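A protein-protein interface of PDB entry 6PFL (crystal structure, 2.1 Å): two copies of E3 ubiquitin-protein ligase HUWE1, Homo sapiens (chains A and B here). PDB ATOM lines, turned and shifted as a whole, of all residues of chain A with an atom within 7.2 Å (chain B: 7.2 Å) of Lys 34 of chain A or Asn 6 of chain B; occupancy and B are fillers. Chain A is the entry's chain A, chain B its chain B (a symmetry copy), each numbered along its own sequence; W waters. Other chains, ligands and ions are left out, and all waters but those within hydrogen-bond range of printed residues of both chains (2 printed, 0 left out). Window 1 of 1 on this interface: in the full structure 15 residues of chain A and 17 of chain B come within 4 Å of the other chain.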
ATOM      1  N   ASN A   4      -6.656 -10.790  16.586  1.00  0.00           N
ATOM      2  CA  ASN A   4      -5.312 -11.035  17.212  1.00  0.00           C
ATOM      3  C   ASN A   4      -5.447 -10.963  18.743  1.00  0.00           C
ATOM      4  O   ASN A   4      -6.565 -11.176  19.241  1.00  0.00           O
ATOM      5  CB  ASN A   4      -4.287 -10.033  16.667  1.00  0.00           C
ATOM      6  N   SER A   5      -4.339 -10.723  19.451  1.00  0.00           N
ATOM      7  CA  SER A   5      -4.245 -10.636  20.938  1.00  0.00           C
ATOM      8  C   SER A   5      -3.085  -9.701  21.303  1.00  0.00           C
ATOM      9  O   SER A   5      -2.359  -9.287  20.379  1.00  0.00           O
ATOM     10  CB  SER A   5      -4.069 -12.009  21.569  1.00  0.00           C
ATOM     11  N   ASN A   6      -2.941  -9.352  22.591  1.00  0.00           N
ATOM     12  CA  ASN A   6      -1.828  -8.493  23.105  1.00  0.00           C
ATOM     13  C   ASN A   6      -0.533  -9.297  23.101  1.00  0.00           C
ATOM     14  O   ASN A   6      -0.591 -10.545  23.151  1.00  0.00           O
ATOM     15  CB  ASN A   6      -2.078  -7.953  24.516  1.00  0.00           C
ATOM     16  CG  ASN A   6      -2.941  -6.711  24.543  1.00  0.00           C
ATOM     17  OD1 ASN A   6      -2.916  -5.911  23.608  1.00  0.00           O
ATOM     18  ND2 ASN A   6      -3.698  -6.544  25.616  1.00  0.00           N
ATOM     19  N   TRP A   8       2.721 -10.336  24.959  1.00  0.00           N
ATOM     20  CA  TRP A   8       3.365 -10.527  26.272  1.00  0.00           C
ATOM     21  C   TRP A   8       4.787 -10.994  26.056  1.00  0.00           C
ATOM     22  O   TRP A   8       4.993 -11.885  25.233  1.00  0.00           O
ATOM     23  CB  TRP A   8       2.568 -11.521  27.097  1.00  0.00           C
ATOM     24  CG  TRP A   8       1.322 -10.921  27.641  1.00  0.00           C
ATOM     25  CD1 TRP A   8       0.091 -10.903  27.058  1.00  0.00           C
ATOM     26  CD2 TRP A   8       1.194 -10.235  28.893  1.00  0.00           C
ATOM     27  NE1 TRP A   8      -0.793 -10.229  27.856  1.00  0.00           N
ATOM     28  CE2 TRP A   8      -0.150  -9.816  28.993  1.00  0.00           C
ATOM     29  CE3 TRP A   8       2.075  -9.969  29.962  1.00  0.00           C
ATOM     30  CZ2 TRP A   8      -0.632  -9.138  30.118  1.00  0.00           C
ATOM     31  CZ3 TRP A   8       1.607  -9.264  31.055  1.00  0.00           C
ATOM     32  CH2 TRP A   8       0.269  -8.858  31.127  1.00  0.00           C
ATOM     33  N   ILE A  29      -2.480 -16.184  28.722  1.00  0.00           N
ATOM     34  CA  ILE A  29      -2.051 -15.056  29.605  1.00  0.00           C
ATOM     35  C   ILE A  29      -2.967 -13.844  29.339  1.00  0.00           C
ATOM     36  O   ILE A  29      -3.428 -13.220  30.295  1.00  0.00           O
ATOM     37  CB  ILE A  29      -0.557 -14.712  29.370  1.00  0.00           C
ATOM     38  CG1 ILE A  29       0.381 -15.821  29.870  1.00  0.00           C
ATOM     39  CG2 ILE A  29      -0.210 -13.352  29.986  1.00  0.00           C
ATOM     40  CD1 ILE A  29       1.823 -15.700  29.356  1.00  0.00           C
ATOM     41  N   ASP A  30      -3.165 -13.495  28.079  1.00  0.00           N
ATOM     42  CA  ASP A  30      -3.895 -12.257  27.706  1.00  0.00           C
ATOM     43  C   ASP A  30      -5.378 -12.421  28.088  1.00  0.00           C
ATOM     44  O   ASP A  30      -5.972 -11.455  28.634  1.00  0.00           O
ATOM     45  CB  ASP A  30      -3.691 -11.923  26.236  1.00  0.00           C
ATOM     46  CG  ASP A  30      -4.026 -10.483  25.919  1.00  0.00           C
ATOM     47  OD1 ASP A  30      -3.333  -9.608  26.445  1.00  0.00           O
ATOM     48  OD2 ASP A  30      -5.007 -10.258  25.194  1.00  0.00           O
ATOM     49  N   SER A  31      -5.917 -13.631  27.931  1.00  0.00           N
ATOM     50  CA  SER A  31      -7.289 -13.996  28.364  1.00  0.00           C
ATOM     51  C   SER A  31      -7.438 -13.785  29.875  1.00  0.00           C
ATOM     52  O   SER A  31      -8.434 -13.160  30.303  1.00  0.00           O
ATOM     53  CB  SER A  31      -7.606 -15.381  27.968  1.00  0.00           C
ATOM     54  OG  SER A  31      -8.932 -15.678  28.301  1.00  0.00           O
ATOM     55  N   ALA A  32      -6.462 -14.230  30.667  1.00  0.00           N
ATOM     56  CA  ALA A  32      -6.488 -14.060  32.136  1.00  0.00           C
ATOM     57  C   ALA A  32      -6.381 -12.566  32.445  1.00  0.00           C
ATOM     58  O   ALA A  32      -7.064 -12.108  33.322  1.00  0.00           O
ATOM     59  CB  ALA A  32      -5.383 -14.858  32.786  1.00  0.00           C
ATOM     60  N   TRP A  33      -5.584 -11.829  31.664  1.00  0.00           N
ATOM     61  CA  TRP A  33      -5.387 -10.366  31.835  1.00  0.00           C
ATOM     62  C   TRP A  33      -6.723  -9.627  31.603  1.00  0.00           C
ATOM     63  O   TRP A  33      -7.191  -8.936  32.526  1.00  0.00           O
ATOM     64  CB  TRP A  33      -4.278  -9.856  30.920  1.00  0.00           C
ATOM     65  CG  TRP A  33      -4.110  -8.367  30.964  1.00  0.00           C
ATOM     66  CD1 TRP A  33      -4.528  -7.462  30.028  1.00  0.00           C
ATOM     67  CD2 TRP A  33      -3.514  -7.600  32.028  1.00  0.00           C
ATOM     68  NE1 TRP A  33      -4.238  -6.188  30.444  1.00  0.00           N
ATOM     69  CE2 TRP A  33      -3.615  -6.242  31.661  1.00  0.00           C
ATOM     70  CE3 TRP A  33      -2.862  -7.932  33.229  1.00  0.00           C
ATOM     71  CZ2 TRP A  33      -3.092  -5.222  32.454  1.00  0.00           C
ATOM     72  CZ3 TRP A  33      -2.373  -6.920  34.028  1.00  0.00           C
ATOM     73  CH2 TRP A  33      -2.474  -5.582  33.634  1.00  0.00           C
ATOM     74  N   LYS A  34      -7.376  -9.882  30.477  1.00  0.00           N
ATOM     75  CA  LYS A  34      -8.696  -9.276  30.128  1.00  0.00           C
ATOM     76  C   LYS A  34      -9.755  -9.593  31.206  1.00  0.00           C
ATOM     77  O   LYS A  34     -10.569  -8.700  31.480  1.00  0.00           O
ATOM     78  CB  LYS A  34      -9.172  -9.761  28.759  1.00  0.00           C
ATOM     79  CG  LYS A  34      -8.202  -9.540  27.607  1.00  0.00           C
ATOM     80  CD  LYS A  34      -7.795  -8.105  27.426  1.00  0.00           C
ATOM     81  CE  LYS A  34      -7.125  -7.852  26.092  1.00  0.00           C
ATOM     82  NZ  LYS A  34      -8.035  -8.159  24.959  1.00  0.00           N
ATOM     83  N   SER A  35      -9.755 -10.795  31.796  1.00  0.00           N
ATOM     84  CA  SER A  35     -10.839 -11.296  32.707  1.00  0.00           C
ATOM     85  C   SER A  35     -10.692 -10.725  34.111  1.00  0.00           C
ATOM     86  O   SER A  35     -11.542 -11.036  34.955  1.00  0.00           O
ATOM     87  CB  SER A  35     -10.871 -12.777  32.753  1.00  0.00           C
ATOM     88  OG  SER A  35     -10.994 -13.306  31.445  1.00  0.00           O
ATOM     89  N   GLY A  36      -9.621  -9.970  34.365  1.00  0.00           N
ATOM     90  CA  GLY A  36      -9.360  -9.324  35.661  1.00  0.00           C
ATOM     91  C   GLY A  36      -8.701 -10.258  36.676  1.00  0.00           C
ATOM     92  O   GLY A  36      -8.538  -9.847  37.817  1.00  0.00           O
ATOM     93  N   GLU A  37      -8.255 -11.443  36.273  1.00  0.00           N
ATOM     94  CA  GLU A  37      -7.485 -12.352  37.178  1.00  0.00           C
ATOM     95  C   GLU A  37      -6.247 -11.593  37.710  1.00  0.00           C
ATOM     96  O   GLU A  37      -5.754 -10.699  37.014  1.00  0.00           O
ATOM     97  CB  GLU A  37      -7.099 -13.609  36.403  1.00  0.00           C
ATOM     98  CG  GLU A  37      -8.285 -14.395  35.885  1.00  0.00           C
ATOM     99  CD  GLU A  37      -9.347 -14.675  36.940  1.00  0.00           C
ATOM    100  OE1 GLU A  37     -10.535 -14.393  36.665  1.00  0.00           O
ATOM    101  OE2 GLU A  37      -8.979 -15.139  38.048  1.00  0.00           O
ATOM    102  N   PHE A  53       0.457 -10.717  38.044  1.00  0.00           N
ATOM    103  CA  PHE A  53       0.175  -9.442  37.327  1.00  0.00           C
ATOM    104  C   PHE A  53       0.435  -8.242  38.255  1.00  0.00           C
ATOM    105  O   PHE A  53       0.744  -7.121  37.765  1.00  0.00           O
ATOM    106  CB  PHE A  53      -1.264  -9.447  36.778  1.00  0.00           C
ATOM    107  CG  PHE A  53      -1.529 -10.401  35.638  1.00  0.00           C
ATOM    108  CD1 PHE A  53      -0.611 -10.585  34.627  1.00  0.00           C
ATOM    109  CD2 PHE A  53      -2.740 -11.077  35.551  1.00  0.00           C
ATOM    110  CE1 PHE A  53      -0.890 -11.410  33.548  1.00  0.00           C
ATOM    111  CE2 PHE A  53      -3.019 -11.908  34.475  1.00  0.00           C
ATOM    112  CZ  PHE A  53      -2.095 -12.075  33.473  1.00  0.00           C
ATOM    113  N   LEU A  73       1.061  -3.072  24.069  1.00  0.00           N
ATOM    114  CA  LEU A  73      -0.249  -2.823  23.427  1.00  0.00           C
ATOM    115  C   LEU A  73      -0.094  -2.825  21.889  1.00  0.00           C
ATOM    116  O   LEU A  73       0.655  -1.962  21.344  1.00  0.00           O
ATOM    117  CB  LEU A  73      -0.784  -1.497  23.957  1.00  0.00           C
ATOM    118  CG  LEU A  73      -0.986  -1.458  25.465  1.00  0.00           C
ATOM    119  CD1 LEU A  73      -1.183  -0.040  25.945  1.00  0.00           C
ATOM    120  CD2 LEU A  73      -2.154  -2.328  25.868  1.00  0.00           C
ATOM    121  N   ARG A  75      -2.213  -1.815  19.745  1.00  0.00           N
ATOM    122  CA  ARG A  75      -2.996  -0.701  19.116  1.00  0.00           C
ATOM    123  C   ARG A  75      -3.522   0.267  20.205  1.00  0.00           C
ATOM    124  O   ARG A  75      -4.194  -0.213  21.103  1.00  0.00           O
ATOM    125  CB  ARG A  75      -4.150  -1.322  18.307  1.00  0.00           C
ATOM    126  CG  ARG A  75      -4.806  -0.375  17.313  1.00  0.00           C
ATOM    127  CD  ARG A  75      -6.026  -0.965  16.593  1.00  0.00           C
ATOM    128  NE  ARG A  75      -6.597   0.049  15.726  1.00  0.00           N
ATOM    129  CZ  ARG A  75      -7.629  -0.133  14.897  1.00  0.00           C
ATOM    130  NH1 ARG A  75      -8.186  -1.331  14.756  1.00  0.00           N
ATOM    131  NH2 ARG A  75      -8.057   0.879  14.169  1.00  0.00           N
ATOM    132  N   ASN B   4     -13.759 -12.361  28.222  1.00  0.00           N
ATOM    133  CA  ASN B   4     -12.354 -11.856  28.269  1.00  0.00           C
ATOM    134  C   ASN B   4     -12.056 -11.045  26.994  1.00  0.00           C
ATOM    135  O   ASN B   4     -11.399 -11.595  26.079  1.00  0.00           O
ATOM    136  CB  ASN B   4     -11.372 -13.021  28.440  1.00  0.00           C
ATOM    137  N   SER B   5     -12.519  -9.785  26.952  1.00  0.00           N
ATOM    138  CA  SER B   5     -12.203  -8.753  25.919  1.00  0.00           C
ATOM    139  C   SER B   5     -12.066  -7.378  26.593  1.00  0.00           C
ATOM    140  O   SER B   5     -12.444  -7.267  27.774  1.00  0.00           O
ATOM    141  CB  SER B   5     -13.261  -8.728  24.814  1.00  0.00           C
ATOM    142  OG  SER B   5     -14.578  -8.792  25.348  1.00  0.00           O
ATOM    143  N   ASN B   6     -11.561  -6.373  25.864  1.00  0.00           N
ATOM    144  CA  ASN B   6     -11.479  -4.944  26.318  1.00  0.00           C
ATOM    145  C   ASN B   6     -12.903  -4.389  26.547  1.00  0.00           C
ATOM    146  O   ASN B   6     -13.859  -4.843  25.843  1.00  0.00           O
ATOM    147  CB  ASN B   6     -10.732  -4.057  25.318  1.00  0.00           C
ATOM    148  CG  ASN B   6      -9.402  -4.627  24.857  1.00  0.00           C
ATOM    149  OD1 ASN B   6      -8.558  -4.978  25.683  1.00  0.00           O
ATOM    150  ND2 ASN B   6      -9.184  -4.685  23.544  1.00  0.00           N
ATOM    151  N   ASN B   7     -13.071  -3.474  27.507  1.00  0.00           N
ATOM    152  CA  ASN B   7     -14.379  -2.822  27.773  1.00  0.00           C
ATOM    153  C   ASN B   7     -14.390  -1.468  27.044  1.00  0.00           C
ATOM    154  O   ASN B   7     -13.550  -0.602  27.350  1.00  0.00           O
ATOM    155  CB  ASN B   7     -14.711  -2.765  29.269  1.00  0.00           C
ATOM    156  CG  ASN B   7     -15.234  -4.090  29.794  1.00  0.00           C
ATOM    157  OD1 ASN B   7     -14.458  -4.929  30.241  1.00  0.00           O
ATOM    158  ND2 ASN B   7     -16.537  -4.315  29.695  1.00  0.00           N
ATOM    159  N   TRP B   8     -15.213  -1.391  26.005  1.00  0.00           N
ATOM    160  CA  TRP B   8     -15.573  -0.164  25.277  1.00  0.00           C
ATOM    161  C   TRP B   8     -16.742   0.518  25.983  1.00  0.00           C
ATOM    162  O   TRP B   8     -17.526  -0.174  26.578  1.00  0.00           O
ATOM    163  CB  TRP B   8     -15.920  -0.557  23.847  1.00  0.00           C
ATOM    164  CG  TRP B   8     -14.716  -1.014  23.105  1.00  0.00           C
ATOM    165  CD1 TRP B   8     -14.148  -2.255  23.121  1.00  0.00           C
ATOM    166  CD2 TRP B   8     -13.837  -0.181  22.342  1.00  0.00           C
ATOM    167  NE1 TRP B   8     -13.005  -2.255  22.369  1.00  0.00           N
ATOM    168  CE2 TRP B   8     -12.773  -0.992  21.905  1.00  0.00           C
ATOM    169  CE3 TRP B   8     -13.861   1.159  21.973  1.00  0.00           C
ATOM    170  CZ2 TRP B   8     -11.763  -0.509  21.080  1.00  0.00           C
ATOM    171  CZ3 TRP B   8     -12.865   1.634  21.158  1.00  0.00           C
ATOM    172  CH2 TRP B   8     -11.818   0.818  20.738  1.00  0.00           C
ATOM    173  N   ASN B  26     -20.033  -5.305  22.676  1.00  0.00           N
ATOM    174  CA  ASN B  26     -18.631  -5.176  23.164  1.00  0.00           C
ATOM    175  C   ASN B  26     -17.710  -6.162  22.436  1.00  0.00           C
ATOM    176  O   ASN B  26     -16.611  -5.750  22.051  1.00  0.00           O
ATOM    177  CB  ASN B  26     -18.518  -5.385  24.669  1.00  0.00           C
ATOM    178  CG  ASN B  26     -17.192  -4.885  25.174  1.00  0.00           C
ATOM    179  OD1 ASN B  26     -17.038  -3.697  25.413  1.00  0.00           O
ATOM    180  ND2 ASN B  26     -16.205  -5.758  25.207  1.00  0.00           N
ATOM    181  N   SER B  27     -18.116  -7.421  22.267  1.00  0.00           N
ATOM    182  CA  SER B  27     -17.282  -8.467  21.585  1.00  0.00           C
ATOM    183  C   SER B  27     -17.134  -8.144  20.092  1.00  0.00           C
ATOM    184  O   SER B  27     -15.994  -8.246  19.544  1.00  0.00           O
ATOM    185  CB  SER B  27     -17.836  -9.843  21.794  1.00  0.00           C
ATOM    186  OG  SER B  27     -17.132 -10.491  22.841  1.00  0.00           O
ATOM    187  N   ILE B  29     -17.279  -5.152  18.651  1.00  0.00           N
ATOM    188  CA  ILE B  29     -16.399  -3.952  18.570  1.00  0.00           C
ATOM    189  C   ILE B  29     -14.949  -4.393  18.818  1.00  0.00           C
ATOM    190  O   ILE B  29     -14.059  -3.998  18.044  1.00  0.00           O
ATOM    191  CB  ILE B  29     -16.847  -2.854  19.559  1.00  0.00           C
ATOM    192  CG1 ILE B  29     -18.219  -2.272  19.195  1.00  0.00           C
ATOM    193  CG2 ILE B  29     -15.784  -1.774  19.657  1.00  0.00           C
ATOM    194  CD1 ILE B  29     -18.830  -1.400  20.284  1.00  0.00           C
ATOM    195  N   ASP B  30     -14.707  -5.161  19.872  1.00  0.00           N
ATOM    196  CA  ASP B  30     -13.320  -5.468  20.308  1.00  0.00           C
ATOM    197  C   ASP B  30     -12.660  -6.375  19.265  1.00  0.00           C
ATOM    198  O   ASP B  30     -11.477  -6.201  19.040  1.00  0.00           O
ATOM    199  CB  ASP B  30     -13.291  -6.068  21.714  1.00  0.00           C
ATOM    200  CG  ASP B  30     -11.949  -5.921  22.411  1.00  0.00           C
ATOM    201  OD1 ASP B  30     -11.286  -4.847  22.236  1.00  0.00           O
ATOM    202  OD2 ASP B  30     -11.583  -6.859  23.145  1.00  0.00           O
ATOM    203  N   SER B  31     -13.419  -7.265  18.613  1.00  0.00           N
ATOM    204  CA  SER B  31     -12.887  -8.180  17.553  1.00  0.00           C
ATOM    205  C   SER B  31     -12.397  -7.346  16.385  1.00  0.00           C
ATOM    206  O   SER B  31     -11.327  -7.663  15.824  1.00  0.00           O
ATOM    207  CB  SER B  31     -13.923  -9.164  17.083  1.00  0.00           C
ATOM    208  OG  SER B  31     -14.029 -10.240  17.989  1.00  0.00           O
ATOM    209  N   TRP B  33     -11.547  -4.099  16.430  1.00  0.00           N
ATOM    210  CA  TRP B  33     -10.375  -3.383  16.977  1.00  0.00           C
ATOM    211  C   TRP B  33      -9.135  -4.280  16.882  1.00  0.00           C
ATOM    212  O   TRP B  33      -8.141  -3.843  16.335  1.00  0.00           O
ATOM    213  CB  TRP B  33     -10.654  -2.986  18.417  1.00  0.00           C
ATOM    214  CG  TRP B  33      -9.491  -2.367  19.101  1.00  0.00           C
ATOM    215  CD1 TRP B  33      -8.702  -2.943  20.052  1.00  0.00           C
ATOM    216  CD2 TRP B  33      -9.007  -1.018  18.935  1.00  0.00           C
ATOM    217  NE1 TRP B  33      -7.751  -2.052  20.477  1.00  0.00           N
ATOM    218  CE2 TRP B  33      -7.896  -0.874  19.795  1.00  0.00           C
ATOM    219  CE3 TRP B  33      -9.414   0.082  18.169  1.00  0.00           C
ATOM    220  CZ2 TRP B  33      -7.201   0.327  19.910  1.00  0.00           C
ATOM    221  CZ3 TRP B  33      -8.713   1.258  18.259  1.00  0.00           C
ATOM    222  CH2 TRP B  33      -7.644   1.391  19.153  1.00  0.00           C
ATOM    223  N   LYS B  34      -9.236  -5.506  17.374  1.00  0.00           N
ATOM    224  CA  LYS B  34      -8.086  -6.439  17.484  1.00  0.00           C
ATOM    225  C   LYS B  34      -7.540  -6.736  16.069  1.00  0.00           C
ATOM    226  O   LYS B  34      -6.344  -6.684  15.923  1.00  0.00           O
ATOM    227  CB  LYS B  34      -8.504  -7.690  18.271  1.00  0.00           C
ATOM    228  CG  LYS B  34      -8.694  -7.472  19.771  1.00  0.00           C
ATOM    229  CD  LYS B  34      -9.378  -8.635  20.507  1.00  0.00           C
ATOM    230  N   LEU B  71     -11.949   3.568  25.045  1.00  0.00           N
ATOM    231  CA  LEU B  71     -11.391   2.254  25.380  1.00  0.00           C
ATOM    232  C   LEU B  71     -10.774   2.372  26.762  1.00  0.00           C
ATOM    233  O   LEU B  71      -9.891   3.189  26.925  1.00  0.00           O
ATOM    234  CB  LEU B  71     -10.350   1.883  24.312  1.00  0.00           C
ATOM    235  CG  LEU B  71      -9.476   0.660  24.608  1.00  0.00           C
ATOM    236  CD1 LEU B  71     -10.311  -0.613  24.796  1.00  0.00           C
ATOM    237  CD2 LEU B  71      -8.463   0.471  23.494  1.00  0.00           C
ATOM    238  N   THR B  72     -11.230   1.593  27.729  1.00  0.00           N
ATOM    239  CA  THR B  72     -10.649   1.627  29.088  1.00  0.00           C
ATOM    240  C   THR B  72      -9.215   1.088  29.018  1.00  0.00           C
ATOM    241  O   THR B  72      -8.958   0.205  28.194  1.00  0.00           O
ATOM    242  CB  THR B  72     -11.521   0.864  30.080  1.00  0.00           C
ATOM    243  OG1 THR B  72     -11.408  -0.481  29.673  1.00  0.00           O
ATOM    244  CG2 THR B  72     -12.972   1.285  30.082  1.00  0.00           C
ATOM    245  N   LEU B  74      -6.356  -0.700  31.318  1.00  0.00           N
ATOM    246  CA  LEU B  74      -6.114  -1.450  32.578  1.00  0.00           C
ATOM    247  C   LEU B  74      -4.697  -1.120  33.063  1.00  0.00           C
ATOM    248  O   LEU B  74      -3.828  -0.874  32.199  1.00  0.00           O
ATOM    249  CB  LEU B  74      -6.325  -2.946  32.318  1.00  0.00           C
ATOM    250  CG  LEU B  74      -7.697  -3.338  31.759  1.00  0.00           C
ATOM    251  CD1 LEU B  74      -7.797  -4.846  31.577  1.00  0.00           C
ATOM    252  CD2 LEU B  74      -8.828  -2.844  32.661  1.00  0.00           C
ATOM    253  N   ARG B  78      -0.947  -4.399  37.713  1.00  0.00           N
ATOM    254  CA  ARG B  78      -2.304  -4.599  38.322  1.00  0.00           C
ATOM    255  C   ARG B  78      -2.231  -4.400  39.837  1.00  0.00           C
ATOM    256  O   ARG B  78      -1.171  -4.694  40.440  1.00  0.00           O
ATOM    257  CB  ARG B  78      -2.851  -5.977  37.966  1.00  0.00           C
ATOM    258  CG  ARG B  78      -4.233  -6.293  38.561  1.00  0.00           C
ATOM    259  CD  ARG B  78      -5.065  -7.220  37.671  1.00  0.00           C
ATOM    260  NE  ARG B  78      -5.154  -6.687  36.312  1.00  0.00           N
ATOM    261  CZ  ARG B  78      -5.621  -7.327  35.234  1.00  0.00           C
ATOM    262  NH1 ARG B  78      -6.009  -8.595  35.282  1.00  0.00           N
ATOM    263  NH2 ARG B  78      -5.670  -6.683  34.085  1.00  0.00           N
HETATM  264  O   HOH W   1      -6.561  -6.325  22.987  1.00  0.00           O
HETATM  265  O   HOH W   2     -10.499  -6.446  29.908  1.00  0.00           O
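Of chain B, only Asn 4 (3.6 Å), Ser 5 (3.8 Å) and Asn 6 (3.2 Å) come within 4 Å of Lys 34 of chain A.
Of the printed residues of chain B, Gly 36 of chain A touches Arg 78 (3.5 Å).
Printed residues of chain B within 4 Å of Glu 37 of chain A: Arg 78.
Printed residues of chain B within 4 Å of Arg 75 of chain A: Trp 33.
Asn 26 of chain B touches none of the printed residues of chain A.
Printed residues of chain A within 4 Å of Lys 34 of chain B: Asn 4.
The nearest residue of chain B that does not touch Lys 34 of chain A is Asp 30 of chain B (4.2 Å).
The nearest residue of chain A that does not touch Asn 6 of chain B is Asn 6 of chain A (5.1 Å).
Printed residues of chain B that touch a printed residue of chain A: Asn 4, Ser 5, Asn 6, Trp 33, Lys 34, Leu 74 and Arg 78.
Hydrophobic or aromatic side chains of chain B within 4 Å of the printed part of chain A: Trp 33 and Leu 74.
Printed residues of chain A that touch a printed residue of chain B: Asn 4, Ser 31, Trp 33, Lys 34, Ser 35, Gly 36, Glu 37, Phe 53 and Arg 75.
Hydrophobic or aromatic side chains of chain A within 4 Å of the printed part of chain B: Trp 33 and Phe 53.
The side-chain carboxylate (OD2) of Asp 30 of chain A lies within salt-bridge range of the side-chain amino group (NZ) of Lys 34 of chain A (3.7 Å).
The side-chain hydroxyl of Ser 35 of chain A sits at hydrogen-bond distance from the backbone carbonyl oxygen of Ser 31 of chain A, 2.8 Å away.
N of Glu 37 of chain A lies within hydrogen-bond range of O of Ala 32 of chain A (3.3 Å).
ND2 of Asn 26 of chain B sits at hydrogen-bond distance from OG of Ser 5 of chain B.
ND2 of Asn 26 of chain B is in hydrogen-bond range of O of Asn 6 of chain B.
The side-chain amide nitrogen (ND2) of Asn 6 of chain B lies within hydrogen-bond range of the side-chain carboxylate (OD1) of Asp 30 of chain B, at 2.5 Å.
Among the printed residues, merely in contact across the chains: Ser 35 of chain A with Asn 4 of chain B (3.0 Å), Gly 36 of chain A with Arg 78 of chain B (3.5 Å), Ser 31 of chain A with Asn 4 of chain B (3.5 Å), Lys 34 of chain A with Asn 4 of chain B (3.6 Å), Lys 34 of chain A with Ser 5 of chain B (3.8 Å), Trp 33 of chain A with Leu 74 of chain B (3.96 Å) and Asn 4 of chain A with Lys 34 of chain B (3.98 Å).
O of Trp 33 of chain A sits at hydrogen-bond distance from NH1 of Arg 78 of chain B (3.0 Å).
The side-chain amide oxygen (OD1) of Asn 6 of chain B lies close to the side-chain amino group (NZ) of Lys 34 of chain A, 3.3 Å away.
The backbone carbonyl oxygen (O) of Glu 37 of chain A is in hydrogen-bond range of the guanidinium group (NH1) of Arg 78 of chain B (2.7 Å).
O of Phe 53 of chain A lies within hydrogen-bond range of N of Arg 78 of chain B.
NH1 of Arg 75 of chain A lies within hydrogen-bond range of O of Trp 33 of chain B, 3.0 Å away.
Water W2 bridges the backbone carbonyl oxygen of Lys 34 of chain A and the backbone carbonyl oxygen of Ser 5 of chain B.
Water W1 bridges the side-chain amino group of Lys 34 of chain A and the side-chain amide nitrogen of Asn 6 of chain B.
Asn 4 of chain A touches Lys 34 of chain B, and with the chains exchanged Lys 34 of chain A touches Asn 4 of chain B.
Ser 31 of chain A touches Asn 4 of chain B, but with the chains exchanged Asn 4 of chain A does not touch Ser 31 of chain B (5.7 Å).
Lys 34 of chain A touches Ser 5 of chain B, but with the chains exchanged Ser 5 of chain A does not touch Lys 34 of chain B (5.3 Å).
Lys 34 of chain A touches Asn 6 of chain B, but with the chains exchanged Asn 6 of chain A does not touch Lys 34 of chain B (6.7 Å).
Positions printed for both chains: 4, 5, 6, 8, 29, 30, 31, 33 and 34.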
